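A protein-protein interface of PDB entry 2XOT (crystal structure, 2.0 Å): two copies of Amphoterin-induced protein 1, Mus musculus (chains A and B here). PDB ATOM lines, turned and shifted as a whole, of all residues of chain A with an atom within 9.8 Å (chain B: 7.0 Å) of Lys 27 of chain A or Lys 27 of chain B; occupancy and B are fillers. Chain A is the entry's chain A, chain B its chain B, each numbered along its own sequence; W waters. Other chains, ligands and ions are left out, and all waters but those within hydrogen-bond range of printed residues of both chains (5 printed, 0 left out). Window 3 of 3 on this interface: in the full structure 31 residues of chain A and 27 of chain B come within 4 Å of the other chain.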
ATOM      1  N   ASN A  15      26.582 -31.754   3.601  1.00  0.00           N
ATOM      2  CA  ASN A  15      25.294 -31.262   4.033  1.00  0.00           C
ATOM      3  C   ASN A  15      24.131 -32.235   3.845  1.00  0.00           C
ATOM      4  O   ASN A  15      22.986 -31.832   3.895  1.00  0.00           O
ATOM      5  CB  ASN A  15      25.023 -29.923   3.336  1.00  0.00           C
ATOM      6  CG  ASN A  15      26.013 -28.859   3.753  1.00  0.00           C
ATOM      7  OD1 ASN A  15      26.723 -28.277   2.932  1.00  0.00           O
ATOM      8  ND2 ASN A  15      26.105 -28.648   5.051  1.00  0.00           N
ATOM      9  N   CYS A  16      24.434 -33.510   3.627  1.00  0.00           N
ATOM     10  CA  CYS A  16      23.420 -34.554   3.454  1.00  0.00           C
ATOM     11  C   CYS A  16      23.597 -35.689   4.465  1.00  0.00           C
ATOM     12  O   CYS A  16      24.708 -35.980   4.946  1.00  0.00           O
ATOM     13  CB  CYS A  16      23.476 -35.124   2.046  1.00  0.00           C
ATOM     14  SG  CYS A  16      23.035 -33.954   0.784  1.00  0.00           S
ATOM     15  N   LEU A  17      22.465 -36.296   4.794  1.00  0.00           N
ATOM     16  CA  LEU A  17      22.407 -37.548   5.492  1.00  0.00           C
ATOM     17  C   LEU A  17      22.107 -38.569   4.400  1.00  0.00           C
ATOM     18  O   LEU A  17      21.132 -38.441   3.671  1.00  0.00           O
ATOM     19  CB  LEU A  17      21.298 -37.474   6.559  1.00  0.00           C
ATOM     20  CG  LEU A  17      21.305 -38.398   7.798  1.00  0.00           C
ATOM     21  CD1 LEU A  17      21.114 -39.863   7.385  1.00  0.00           C
ATOM     22  CD2 LEU A  17      22.557 -38.203   8.651  1.00  0.00           C
ATOM     23  N   LEU A  23      18.848 -39.379   0.036  1.00  0.00           N
ATOM     24  CA  LEU A  23      19.707 -38.277   0.509  1.00  0.00           C
ATOM     25  C   LEU A  23      18.823 -37.234   1.163  1.00  0.00           C
ATOM     26  O   LEU A  23      17.977 -36.606   0.503  1.00  0.00           O
ATOM     27  CB  LEU A  23      20.489 -37.619  -0.621  1.00  0.00           C
ATOM     28  CG  LEU A  23      21.885 -38.138  -0.953  1.00  0.00           C
ATOM     29  CD1 LEU A  23      21.894 -39.661  -1.198  1.00  0.00           C
ATOM     30  CD2 LEU A  23      22.412 -37.337  -2.186  1.00  0.00           C
ATOM     31  N   SER A  24      19.028 -37.063   2.455  1.00  0.00           N
ATOM     32  CA  SER A  24      18.244 -36.171   3.252  1.00  0.00           C
ATOM     33  C   SER A  24      19.162 -34.993   3.471  1.00  0.00           C
ATOM     34  O   SER A  24      20.085 -35.081   4.255  1.00  0.00           O
ATOM     35  CB  SER A  24      17.894 -36.846   4.577  1.00  0.00           C
ATOM     36  OG  SER A  24      16.909 -36.115   5.280  1.00  0.00           O
ATOM     37  N   CYS A  25      18.928 -33.925   2.706  1.00  0.00           N
ATOM     38  CA  CYS A  25      19.744 -32.716   2.742  1.00  0.00           C
ATOM     39  C   CYS A  25      18.881 -31.516   3.055  1.00  0.00           C
ATOM     40  O   CYS A  25      19.073 -30.458   2.482  1.00  0.00           O
ATOM     41  CB  CYS A  25      20.423 -32.508   1.390  1.00  0.00           C
ATOM     42  SG  CYS A  25      21.032 -34.009   0.619  1.00  0.00           S
ATOM     43  N   SER A  26      17.911 -31.679   3.947  1.00  0.00           N
ATOM     44  CA  SER A  26      16.982 -30.615   4.235  1.00  0.00           C
ATOM     45  C   SER A  26      17.448 -29.763   5.411  1.00  0.00           C
ATOM     46  O   SER A  26      18.207 -30.228   6.261  1.00  0.00           O
ATOM     47  CB  SER A  26      15.601 -31.167   4.550  1.00  0.00           C
ATOM     48  OG  SER A  26      15.586 -31.775   5.826  1.00  0.00           O
ATOM     49  N   LYS A  27      16.940 -28.534   5.447  1.00  0.00           N
ATOM     50  CA  LYS A  27      17.188 -27.598   6.527  1.00  0.00           C
ATOM     51  C   LYS A  27      18.688 -27.413   6.777  1.00  0.00           C
ATOM     52  O   LYS A  27      19.144 -27.477   7.902  1.00  0.00           O
ATOM     53  CB  LYS A  27      16.445 -28.020   7.801  1.00  0.00           C
ATOM     54  CG  LYS A  27      15.992 -26.820   8.656  1.00  0.00           C
ATOM     55  CD  LYS A  27      15.523 -27.186  10.055  1.00  0.00           C
ATOM     56  CE  LYS A  27      16.557 -28.043  10.771  1.00  0.00           C
ATOM     57  NZ  LYS A  27      16.360 -28.131  12.256  1.00  0.00           N
ATOM     58  N   GLN A  28      19.435 -27.158   5.704  1.00  0.00           N
ATOM     59  CA  GLN A  28      20.891 -26.927   5.771  1.00  0.00           C
ATOM     60  C   GLN A  28      21.317 -25.537   5.257  1.00  0.00           C
ATOM     61  O   GLN A  28      22.481 -25.337   4.916  1.00  0.00           O
ATOM     62  CB  GLN A  28      21.636 -28.010   4.971  1.00  0.00           C
ATOM     63  CG  GLN A  28      21.507 -29.390   5.527  1.00  0.00           C
ATOM     64  CD  GLN A  28      22.107 -29.500   6.890  1.00  0.00           C
ATOM     65  OE1 GLN A  28      23.231 -29.074   7.117  1.00  0.00           O
ATOM     66  NE2 GLN A  28      21.353 -30.046   7.822  1.00  0.00           N
ATOM     67  N   GLN A  29      20.366 -24.608   5.168  1.00  0.00           N
ATOM     68  CA  GLN A  29      20.633 -23.228   4.725  1.00  0.00           C
ATOM     69  C   GLN A  29      21.287 -23.122   3.341  1.00  0.00           C
ATOM     70  O   GLN A  29      21.966 -22.140   3.049  1.00  0.00           O
ATOM     71  CB  GLN A  29      21.515 -22.493   5.759  1.00  0.00           C
ATOM     72  CG  GLN A  29      20.948 -22.464   7.180  1.00  0.00           C
ATOM     73  CD  GLN A  29      21.148 -23.747   7.957  1.00  0.00           C
ATOM     74  OE1 GLN A  29      22.239 -24.302   7.990  1.00  0.00           O
ATOM     75  NE2 GLN A  29      20.096 -24.212   8.606  1.00  0.00           N
ATOM     76  N   LEU A  30      21.053 -24.116   2.485  1.00  0.00           N
ATOM     77  CA  LEU A  30      21.834 -24.258   1.261  1.00  0.00           C
ATOM     78  C   LEU A  30      21.368 -23.280   0.190  1.00  0.00           C
ATOM     79  O   LEU A  30      20.188 -23.249  -0.149  1.00  0.00           O
ATOM     80  CB  LEU A  30      21.774 -25.686   0.709  1.00  0.00           C
ATOM     81  CG  LEU A  30      22.436 -26.773   1.544  1.00  0.00           C
ATOM     82  CD1 LEU A  30      22.032 -28.146   1.014  1.00  0.00           C
ATOM     83  CD2 LEU A  30      23.955 -26.622   1.580  1.00  0.00           C
ATOM     84  N   PRO A  31      22.291 -22.463  -0.341  1.00  0.00           N
ATOM     85  CA  PRO A  31      21.953 -21.571  -1.431  1.00  0.00           C
ATOM     86  C   PRO A  31      22.106 -22.246  -2.816  1.00  0.00           C
ATOM     87  O   PRO A  31      21.597 -21.745  -3.799  1.00  0.00           O
ATOM     88  CB  PRO A  31      22.967 -20.443  -1.248  1.00  0.00           C
ATOM     89  CG  PRO A  31      24.178 -21.132  -0.795  1.00  0.00           C
ATOM     90  CD  PRO A  31      23.697 -22.289   0.072  1.00  0.00           C
ATOM     91  N   ASP A  45      16.002 -35.005  -1.047  1.00  0.00           N
ATOM     92  CA  ASP A  45      15.221 -34.088  -0.227  1.00  0.00           C
ATOM     93  C   ASP A  45      16.079 -32.875   0.023  1.00  0.00           C
ATOM     94  O   ASP A  45      17.044 -32.949   0.782  1.00  0.00           O
ATOM     95  CB  ASP A  45      14.829 -34.748   1.102  1.00  0.00           C
ATOM     96  CG  ASP A  45      13.920 -33.865   1.953  1.00  0.00           C
ATOM     97  OD1 ASP A  45      13.612 -32.725   1.556  1.00  0.00           O
ATOM     98  OD2 ASP A  45      13.538 -34.299   3.053  1.00  0.00           O
ATOM     99  N   LEU A  46      15.742 -31.785  -0.650  1.00  0.00           N
ATOM    100  CA  LEU A  46      16.428 -30.500  -0.521  1.00  0.00           C
ATOM    101  C   LEU A  46      15.468 -29.450   0.039  1.00  0.00           C
ATOM    102  O   LEU A  46      15.672 -28.246  -0.126  1.00  0.00           O
ATOM    103  CB  LEU A  46      16.989 -30.057  -1.884  1.00  0.00           C
ATOM    104  CG  LEU A  46      18.320 -30.677  -2.279  1.00  0.00           C
ATOM    105  CD1 LEU A  46      18.602 -30.437  -3.731  1.00  0.00           C
ATOM    106  CD2 LEU A  46      19.491 -30.152  -1.388  1.00  0.00           C
ATOM    107  N   SER A  47      14.412 -29.897   0.715  1.00  0.00           N
ATOM    108  CA  SER A  47      13.411 -28.965   1.223  1.00  0.00           C
ATOM    109  C   SER A  47      13.973 -28.103   2.376  1.00  0.00           C
ATOM    110  O   SER A  47      14.926 -28.501   3.053  1.00  0.00           O
ATOM    111  CB  SER A  47      12.197 -29.728   1.734  1.00  0.00           C
ATOM    112  OG  SER A  47      12.570 -30.552   2.829  1.00  0.00           O
ATOM    113  N   HIS A  48      13.349 -26.945   2.603  1.00  0.00           N
ATOM    114  CA  HIS A  48      13.702 -26.037   3.703  1.00  0.00           C
ATOM    115  C   HIS A  48      15.135 -25.565   3.593  1.00  0.00           C
ATOM    116  O   HIS A  48      15.883 -25.544   4.560  1.00  0.00           O
ATOM    117  CB  HIS A  48      13.424 -26.667   5.062  1.00  0.00           C
ATOM    118  CG  HIS A  48      11.976 -26.962   5.295  1.00  0.00           C
ATOM    119  ND1 HIS A  48      11.062 -25.985   5.635  1.00  0.00           N
ATOM    120  CD2 HIS A  48      11.277 -28.121   5.218  1.00  0.00           C
ATOM    121  CE1 HIS A  48       9.870 -26.532   5.780  1.00  0.00           C
ATOM    122  NE2 HIS A  48       9.967 -27.828   5.516  1.00  0.00           N
ATOM    123  N   ASN A  49      15.517 -25.186   2.383  1.00  0.00           N
ATOM    124  CA  ASN A  49      16.823 -24.617   2.159  1.00  0.00           C
ATOM    125  C   ASN A  49      16.651 -23.189   1.634  1.00  0.00           C
ATOM    126  O   ASN A  49      15.589 -22.578   1.787  1.00  0.00           O
ATOM    127  CB  ASN A  49      17.651 -25.523   1.241  1.00  0.00           C
ATOM    128  CG  ASN A  49      18.222 -26.712   1.976  1.00  0.00           C
ATOM    129  OD1 ASN A  49      17.889 -27.867   1.677  1.00  0.00           O
ATOM    130  ND2 ASN A  49      19.069 -26.447   2.948  1.00  0.00           N
ATOM    131  N   ASN A  50      17.691 -22.652   1.032  1.00  0.00           N
ATOM    132  CA  ASN A  50      17.647 -21.298   0.586  1.00  0.00           C
ATOM    133  C   ASN A  50      18.001 -21.193  -0.900  1.00  0.00           C
ATOM    134  O   ASN A  50      18.670 -20.251  -1.329  1.00  0.00           O
ATOM    135  CB  ASN A  50      18.622 -20.528   1.445  1.00  0.00           C
ATOM    136  CG  ASN A  50      18.527 -19.066   1.254  1.00  0.00           C
ATOM    137  OD1 ASN A  50      17.466 -18.511   0.938  1.00  0.00           O
ATOM    138  ND2 ASN A  50      19.650 -18.405   1.444  1.00  0.00           N
ATOM    139  N   LEU A  51      17.542 -22.170  -1.682  1.00  0.00           N
ATOM    140  CA  LEU A  51      17.780 -22.167  -3.130  1.00  0.00           C
ATOM    141  C   LEU A  51      16.901 -21.095  -3.780  1.00  0.00           C
ATOM    142  O   LEU A  51      15.759 -20.897  -3.375  1.00  0.00           O
ATOM    143  CB  LEU A  51      17.490 -23.541  -3.730  1.00  0.00           C
ATOM    144  CG  LEU A  51      18.187 -24.725  -3.060  1.00  0.00           C
ATOM    145  CD1 LEU A  51      17.544 -26.013  -3.527  1.00  0.00           C
ATOM    146  CD2 LEU A  51      19.654 -24.715  -3.383  1.00  0.00           C
ATOM    147  N   LEU A  70      12.551 -33.303  -3.958  1.00  0.00           N
ATOM    148  CA  LEU A  70      11.782 -32.459  -3.016  1.00  0.00           C
ATOM    149  C   LEU A  70      12.517 -31.140  -2.806  1.00  0.00           C
ATOM    150  O   LEU A  70      13.629 -31.121  -2.268  1.00  0.00           O
ATOM    151  CB  LEU A  70      11.575 -33.181  -1.682  1.00  0.00           C
ATOM    152  CG  LEU A  70      11.083 -34.649  -1.823  1.00  0.00           C
ATOM    153  CD1 LEU A  70      11.003 -35.355  -0.450  1.00  0.00           C
ATOM    154  CD2 LEU A  70       9.750 -34.738  -2.585  1.00  0.00           C
ATOM    155  N   LEU A  71      11.884 -30.058  -3.247  1.00  0.00           N
ATOM    156  CA  LEU A  71      12.466 -28.715  -3.223  1.00  0.00           C
ATOM    157  C   LEU A  71      11.543 -27.688  -2.567  1.00  0.00           C
ATOM    158  O   LEU A  71      11.697 -26.471  -2.763  1.00  0.00           O
ATOM    159  CB  LEU A  71      12.783 -28.268  -4.644  1.00  0.00           C
ATOM    160  CG  LEU A  71      13.985 -28.938  -5.286  1.00  0.00           C
ATOM    161  CD1 LEU A  71      13.887 -28.881  -6.836  1.00  0.00           C
ATOM    162  CD2 LEU A  71      15.289 -28.304  -4.783  1.00  0.00           C
ATOM    163  N   SER A  72      10.598 -28.157  -1.771  1.00  0.00           N
ATOM    164  CA  SER A  72       9.667 -27.245  -1.144  1.00  0.00           C
ATOM    165  C   SER A  72      10.374 -26.362  -0.117  1.00  0.00           C
ATOM    166  O   SER A  72      11.490 -26.666   0.340  1.00  0.00           O
ATOM    167  CB  SER A  72       8.494 -27.991  -0.500  1.00  0.00           C
ATOM    168  OG  SER A  72       8.950 -28.758   0.599  1.00  0.00           O
ATOM    169  N   HIS A  73       9.725 -25.251   0.212  1.00  0.00           N
ATOM    170  CA  HIS A  73      10.253 -24.285   1.178  1.00  0.00           C
ATOM    171  C   HIS A  73      11.677 -23.903   0.853  1.00  0.00           C
ATOM    172  O   HIS A  73      12.577 -24.103   1.657  1.00  0.00           O
ATOM    173  CB  HIS A  73      10.153 -24.843   2.592  1.00  0.00           C
ATOM    174  CG  HIS A  73       8.752 -25.091   3.028  1.00  0.00           C
ATOM    175  ND1 HIS A  73       7.934 -24.090   3.496  1.00  0.00           N
ATOM    176  CD2 HIS A  73       8.011 -26.223   3.039  1.00  0.00           C
ATOM    177  CE1 HIS A  73       6.758 -24.598   3.810  1.00  0.00           C
ATOM    178  NE2 HIS A  73       6.779 -25.890   3.538  1.00  0.00           N
ATOM    179  N   ASN A  74      11.870 -23.413  -0.369  1.00  0.00           N
ATOM    180  CA  ASN A  74      13.075 -22.716  -0.775  1.00  0.00           C
ATOM    181  C   ASN A  74      12.654 -21.326  -1.280  1.00  0.00           C
ATOM    182  O   ASN A  74      11.516 -20.908  -1.041  1.00  0.00           O
ATOM    183  CB  ASN A  74      13.806 -23.556  -1.808  1.00  0.00           C
ATOM    184  CG  ASN A  74      14.581 -24.690  -1.169  1.00  0.00           C
ATOM    185  OD1 ASN A  74      14.103 -25.821  -1.044  1.00  0.00           O
ATOM    186  ND2 ASN A  74      15.775 -24.377  -0.718  1.00  0.00           N
ATOM    187  N   HIS A  75      13.533 -20.593  -1.945  1.00  0.00           N
ATOM    188  CA  HIS A  75      13.138 -19.295  -2.493  1.00  0.00           C
ATOM    189  C   HIS A  75      13.240 -19.292  -4.011  1.00  0.00           C
ATOM    190  O   HIS A  75      13.658 -18.311  -4.602  1.00  0.00           O
ATOM    191  CB  HIS A  75      13.957 -18.176  -1.822  1.00  0.00           C
ATOM    192  CG  HIS A  75      13.767 -18.143  -0.342  1.00  0.00           C
ATOM    193  ND1 HIS A  75      14.783 -18.410   0.544  1.00  0.00           N
ATOM    194  CD2 HIS A  75      12.652 -17.971   0.407  1.00  0.00           C
ATOM    195  CE1 HIS A  75      14.314 -18.364   1.781  1.00  0.00           C
ATOM    196  NE2 HIS A  75      13.020 -18.100   1.726  1.00  0.00           N
ATOM    197  N   CYS B  25       2.255 -29.096   7.202  1.00  0.00           N
ATOM    198  CA  CYS B  25       2.322 -28.467   8.524  1.00  0.00           C
ATOM    199  C   CYS B  25       3.753 -28.552   9.117  1.00  0.00           C
ATOM    200  O   CYS B  25       3.943 -28.763  10.324  1.00  0.00           O
ATOM    201  CB  CYS B  25       1.308 -29.123   9.466  1.00  0.00           C
ATOM    202  SG  CYS B  25      -0.277 -29.608   8.742  1.00  0.00           S
ATOM    203  N   SER B  26       4.753 -28.371   8.253  1.00  0.00           N
ATOM    204  CA  SER B  26       6.138 -28.608   8.606  1.00  0.00           C
ATOM    205  C   SER B  26       6.792 -27.345   9.123  1.00  0.00           C
ATOM    206  O   SER B  26       6.379 -26.236   8.770  1.00  0.00           O
ATOM    207  CB  SER B  26       6.915 -29.113   7.383  1.00  0.00           C
ATOM    208  OG  SER B  26       7.138 -28.077   6.452  1.00  0.00           O
ATOM    209  N   LYS B  27       7.834 -27.549   9.926  1.00  0.00           N
ATOM    210  CA  LYS B  27       8.716 -26.500  10.443  1.00  0.00           C
ATOM    211  C   LYS B  27       8.012 -25.356  11.182  1.00  0.00           C
ATOM    212  O   LYS B  27       8.347 -24.186  11.012  1.00  0.00           O
ATOM    213  CB  LYS B  27       9.657 -25.993   9.345  1.00  0.00           C
ATOM    214  CG  LYS B  27      10.910 -25.364   9.891  1.00  0.00           C
ATOM    215  CD  LYS B  27      11.942 -25.134   8.824  1.00  0.00           C
ATOM    216  CE  LYS B  27      12.775 -23.909   9.124  1.00  0.00           C
ATOM    217  NZ  LYS B  27      13.960 -23.804   8.176  1.00  0.00           N
ATOM    218  N   GLN B  28       7.075 -25.732  12.049  1.00  0.00           N
ATOM    219  CA  GLN B  28       6.275 -24.809  12.848  1.00  0.00           C
ATOM    220  C   GLN B  28       6.532 -25.038  14.331  1.00  0.00           C
ATOM    221  O   GLN B  28       5.692 -24.689  15.161  1.00  0.00           O
ATOM    222  CB  GLN B  28       4.793 -25.080  12.615  1.00  0.00           C
ATOM    223  CG  GLN B  28       4.292 -24.913  11.198  1.00  0.00           C
ATOM    224  CD  GLN B  28       4.221 -23.479  10.774  1.00  0.00           C
ATOM    225  OE1 GLN B  28       3.751 -22.620  11.528  1.00  0.00           O
ATOM    226  NE2 GLN B  28       4.681 -23.198   9.557  1.00  0.00           N
ATOM    227  N   GLN B  29       7.657 -25.676  14.651  1.00  0.00           N
ATOM    228  CA  GLN B  29       7.955 -26.180  16.001  1.00  0.00           C
ATOM    229  C   GLN B  29       6.752 -26.637  16.843  1.00  0.00           C
ATOM    230  O   GLN B  29       6.682 -26.345  18.033  1.00  0.00           O
ATOM    231  CB  GLN B  29       8.806 -25.134  16.776  1.00  0.00           C
ATOM    232  N   LEU B  30       5.836 -27.389  16.237  1.00  0.00           N
ATOM    233  CA  LEU B  30       4.667 -27.926  16.936  1.00  0.00           C
ATOM    234  C   LEU B  30       5.078 -28.995  17.939  1.00  0.00           C
ATOM    235  O   LEU B  30       5.837 -29.905  17.587  1.00  0.00           O
ATOM    236  CB  LEU B  30       3.673 -28.554  15.957  1.00  0.00           C
ATOM    237  CG  LEU B  30       3.087 -27.671  14.867  1.00  0.00           C
ATOM    238  CD1 LEU B  30       2.211 -28.528  13.935  1.00  0.00           C
ATOM    239  CD2 LEU B  30       2.304 -26.509  15.466  1.00  0.00           C
ATOM    240  N   ASP B  45       2.224 -33.818   6.187  1.00  0.00           N
ATOM    241  CA  ASP B  45       3.637 -33.498   6.443  1.00  0.00           C
ATOM    242  C   ASP B  45       3.790 -32.730   7.738  1.00  0.00           C
ATOM    243  O   ASP B  45       3.467 -31.550   7.760  1.00  0.00           O
ATOM    244  CB  ASP B  45       4.208 -32.640   5.301  1.00  0.00           C
ATOM    245  CG  ASP B  45       5.677 -32.335   5.476  1.00  0.00           C
ATOM    246  OD1 ASP B  45       6.333 -32.832   6.419  1.00  0.00           O
ATOM    247  OD2 ASP B  45       6.198 -31.585   4.637  1.00  0.00           O
ATOM    248  N   LEU B  46       4.279 -33.414   8.786  1.00  0.00           N
ATOM    249  CA  LEU B  46       4.509 -32.829  10.103  1.00  0.00           C
ATOM    250  C   LEU B  46       5.993 -32.885  10.418  1.00  0.00           C
ATOM    251  O   LEU B  46       6.399 -32.918  11.592  1.00  0.00           O
ATOM    252  CB  LEU B  46       3.748 -33.594  11.163  1.00  0.00           C
ATOM    253  CG  LEU B  46       2.233 -33.398  11.125  1.00  0.00           C
ATOM    254  CD1 LEU B  46       1.523 -34.611  11.677  1.00  0.00           C
ATOM    255  CD2 LEU B  46       1.867 -32.106  11.877  1.00  0.00           C
ATOM    256  N   SER B  47       6.810 -32.907   9.372  1.00  0.00           N
ATOM    257  CA  SER B  47       8.236 -32.988   9.544  1.00  0.00           C
ATOM    258  C   SER B  47       8.789 -31.676  10.102  1.00  0.00           C
ATOM    259  O   SER B  47       8.128 -30.638  10.023  1.00  0.00           O
ATOM    260  CB  SER B  47       8.921 -33.361   8.219  1.00  0.00           C
ATOM    261  OG  SER B  47       8.711 -32.374   7.241  1.00  0.00           O
ATOM    262  N   HIS B  48       9.980 -31.763  10.693  1.00  0.00           N
ATOM    263  CA  HIS B  48      10.693 -30.654  11.301  1.00  0.00           C
ATOM    264  C   HIS B  48       9.832 -29.938  12.351  1.00  0.00           C
ATOM    265  O   HIS B  48       9.668 -28.719  12.311  1.00  0.00           O
ATOM    266  CB  HIS B  48      11.202 -29.669  10.247  1.00  0.00           C
ATOM    267  CG  HIS B  48      12.200 -30.243   9.295  1.00  0.00           C
ATOM    268  ND1 HIS B  48      13.532 -30.401   9.608  1.00  0.00           N
ATOM    269  CD2 HIS B  48      12.066 -30.658   8.014  1.00  0.00           C
ATOM    270  CE1 HIS B  48      14.173 -30.901   8.564  1.00  0.00           C
ATOM    271  NE2 HIS B  48      13.305 -31.065   7.582  1.00  0.00           N
ATOM    272  N   ASN B  49       9.283 -30.701  13.288  1.00  0.00           N
ATOM    273  CA  ASN B  49       8.516 -30.126  14.399  1.00  0.00           C
ATOM    274  C   ASN B  49       9.114 -30.625  15.722  1.00  0.00           C
ATOM    275  O   ASN B  49      10.271 -31.061  15.759  1.00  0.00           O
ATOM    276  CB  ASN B  49       7.022 -30.488  14.258  1.00  0.00           C
ATOM    277  CG  ASN B  49       6.291 -29.591  13.303  1.00  0.00           C
ATOM    278  OD1 ASN B  49       5.675 -30.046  12.330  1.00  0.00           O
ATOM    279  ND2 ASN B  49       6.344 -28.305  13.570  1.00  0.00           N
ATOM    280  N   HIS B  73      12.489 -35.641  11.428  1.00  0.00           N
ATOM    281  CA  HIS B  73      13.043 -34.445  12.064  1.00  0.00           C
ATOM    282  C   HIS B  73      12.118 -33.905  13.154  1.00  0.00           C
ATOM    283  O   HIS B  73      11.798 -32.718  13.208  1.00  0.00           O
ATOM    284  CB  HIS B  73      13.393 -33.374  11.024  1.00  0.00           C
ATOM    285  CG  HIS B  73      14.565 -33.736  10.184  1.00  0.00           C
ATOM    286  ND1 HIS B  73      15.858 -33.698  10.662  1.00  0.00           N
ATOM    287  CD2 HIS B  73      14.645 -34.189   8.913  1.00  0.00           C
ATOM    288  CE1 HIS B  73      16.685 -34.098   9.713  1.00  0.00           C
ATOM    289  NE2 HIS B  73      15.972 -34.395   8.640  1.00  0.00           N
HETATM  290  O   HOH W   1      12.578 -33.064   5.393  1.00  0.00           O
HETATM  291  O   HOH W   2      17.340 -23.188   8.540  1.00  0.00           O
HETATM  292  O   HOH W   3      10.745 -31.121   5.260  1.00  0.00           O
HETATM  293  O   HOH W   4       8.628 -30.355   4.330  1.00  0.00           O
HETATM  294  O   HOH W   5      15.430 -37.632   7.894  1.00  0.00           O
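Hydrophobic or aromatic side chains of chain B that line the printed part of chain A: His 48 and His 73.
Printed residues of chain A that touch a printed residue of chain B: Ser 24, Ser 26, Lys 27, His 48 and His 73.
Hydrophobic or aromatic side chains of chain A that line the printed part of chain B: His 48 and His 73.
Among the printed residues, no Asp or Glu carboxylate lies within 4 Å of a Lys or Arg side-chain nitrogen of the other chain.
Among the printed residues, merely in contact across the chains: His 48 of chain A with Lys 27 of chain B (3.4 Å), His 73 of chain A with Ser 26 of chain B (3.7 Å), Lys 27 of chain A with Lys 27 of chain B (3.7 Å), Lys 27 of chain A with His 48 of chain B (3.7 Å), His 48 of chain A with His 48 of chain B (3.9 Å), Ser 26 of chain A with His 73 of chain B (3.9 Å) and Ser 24 of chain A with His 73 of chain B (3.9 Å).
N of Leu 17 of chain A is in hydrogen-bond range of O of Ser 24 of chain A.
The backbone carbonyl oxygen (O) of Lys 27 of chain A sits at hydrogen-bond distance from the side-chain amide nitrogen (NE2) of Gln 29 of chain A, 3.5 Å away.
The backbone NH (N) of Lys 27 of chain A lies close to the backbone carbonyl oxygen (O) of His 48 of chain A.
N of His 48 of chain A lies within hydrogen-bond range of O of Ser 72 of chain A.
O of His 48 of chain B sits close to N of Lys 27 of chain B (3.2 Å).
N of His 48 of chain B sits close to O of His 73 of chain B (3.2 Å).
Of chain B, only Lys 27 (3.7 Å) and His 48 (3.7 Å) come within 4 Å of Lys 27 of chain A.
Printed residues of chain B within 4 Å of His 73 of chain A: Ser 26 (3.7 Å).
Printed residues of chain A within 4 Å of Ser 26 of chain B: His 48 (3.0 Å) and His 73 (3.7 Å).
Lys 27 of chain B touches two residues of chain A.
No residue of chain A comes within 4 Å of Gln 28 of chain B.
Printed residues of chain A within 4 Å of His 48 of chain B: Ser 26 (3.0 Å), Lys 27 (3.7 Å) and His 48 (3.9 Å).
Of the printed residues of chain A, His 73 of chain B touches Ser 24 and Ser 26.
The nearest printed residue of chain A that does not touch Lys 27 of chain B is Asn 49 of chain A (6.2 Å).
Ser 26 of chain A touches His 73 of chain B, and with the chains exchanged His 73 of chain A touches Ser 26 of chain B.
Lys 27 of chain B touches its own counterpart, Lys 27 of chain A.
Lys 27 of chain A touches His 48 of chain B, and with the chains exchanged His 48 of chain A touches Lys 27 of chain B.
His 48 of chain B touches its own counterpart, His 48 of chain A.
Positions printed for both chains: 25, 26, 27, 28, 29, 30, 45, 46, 47, 48, 49 and 73.
Of the 9 pairs that touch across the chains among the printed residues, 8 have their exchanged pair printed and touching as well.
Water W4 lies within hydrogen-bond range of the side-chain carboxylate of Asp 45 of chain B (2.7 Å), a ring nitrogen (NE2) of His 48 of chain A (3.1 Å) and the side-chain hydroxyl of Ser 26 of chain B (3.5 Å).
Water W1 lies within hydrogen-bond range of the side-chain carboxylate (OD2) of Asp 45 of chain A, a ring nitrogen (NE2) of His 48 of chain B and the side-chain hydroxyl (OG) of Ser 26 of chain A.
Water W2 bridges the side-chain amide nitrogen of Gln 29 of chain A (2.9 Å) and the side-chain amino group of Lys 27 of chain B (3.5 Å).
Water W3 lies within hydrogen-bond range of OG of Ser 47 of chain A (3.1 Å), OG of Ser 47 of chain B (3.1 Å), NE2 of His 48 of chain A (3.4 Å) and NE2 of His 48 of chain B (3.5 Å).
Water W5 lies within hydrogen-bond range of the side-chain hydroxyl of Ser 24 of chain A (3.4 Å) and a ring nitrogen (NE2) of His 73 of chain B (3.4 Å).
OG of Ser 26 of chain A is in hydrogen-bond range of NE2 of His 48 of chain B, at 3.0 Å.
NE2 of His 48 of chain A is in hydrogen-bond range of OG of Ser 26 of chain B (3.0 Å).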
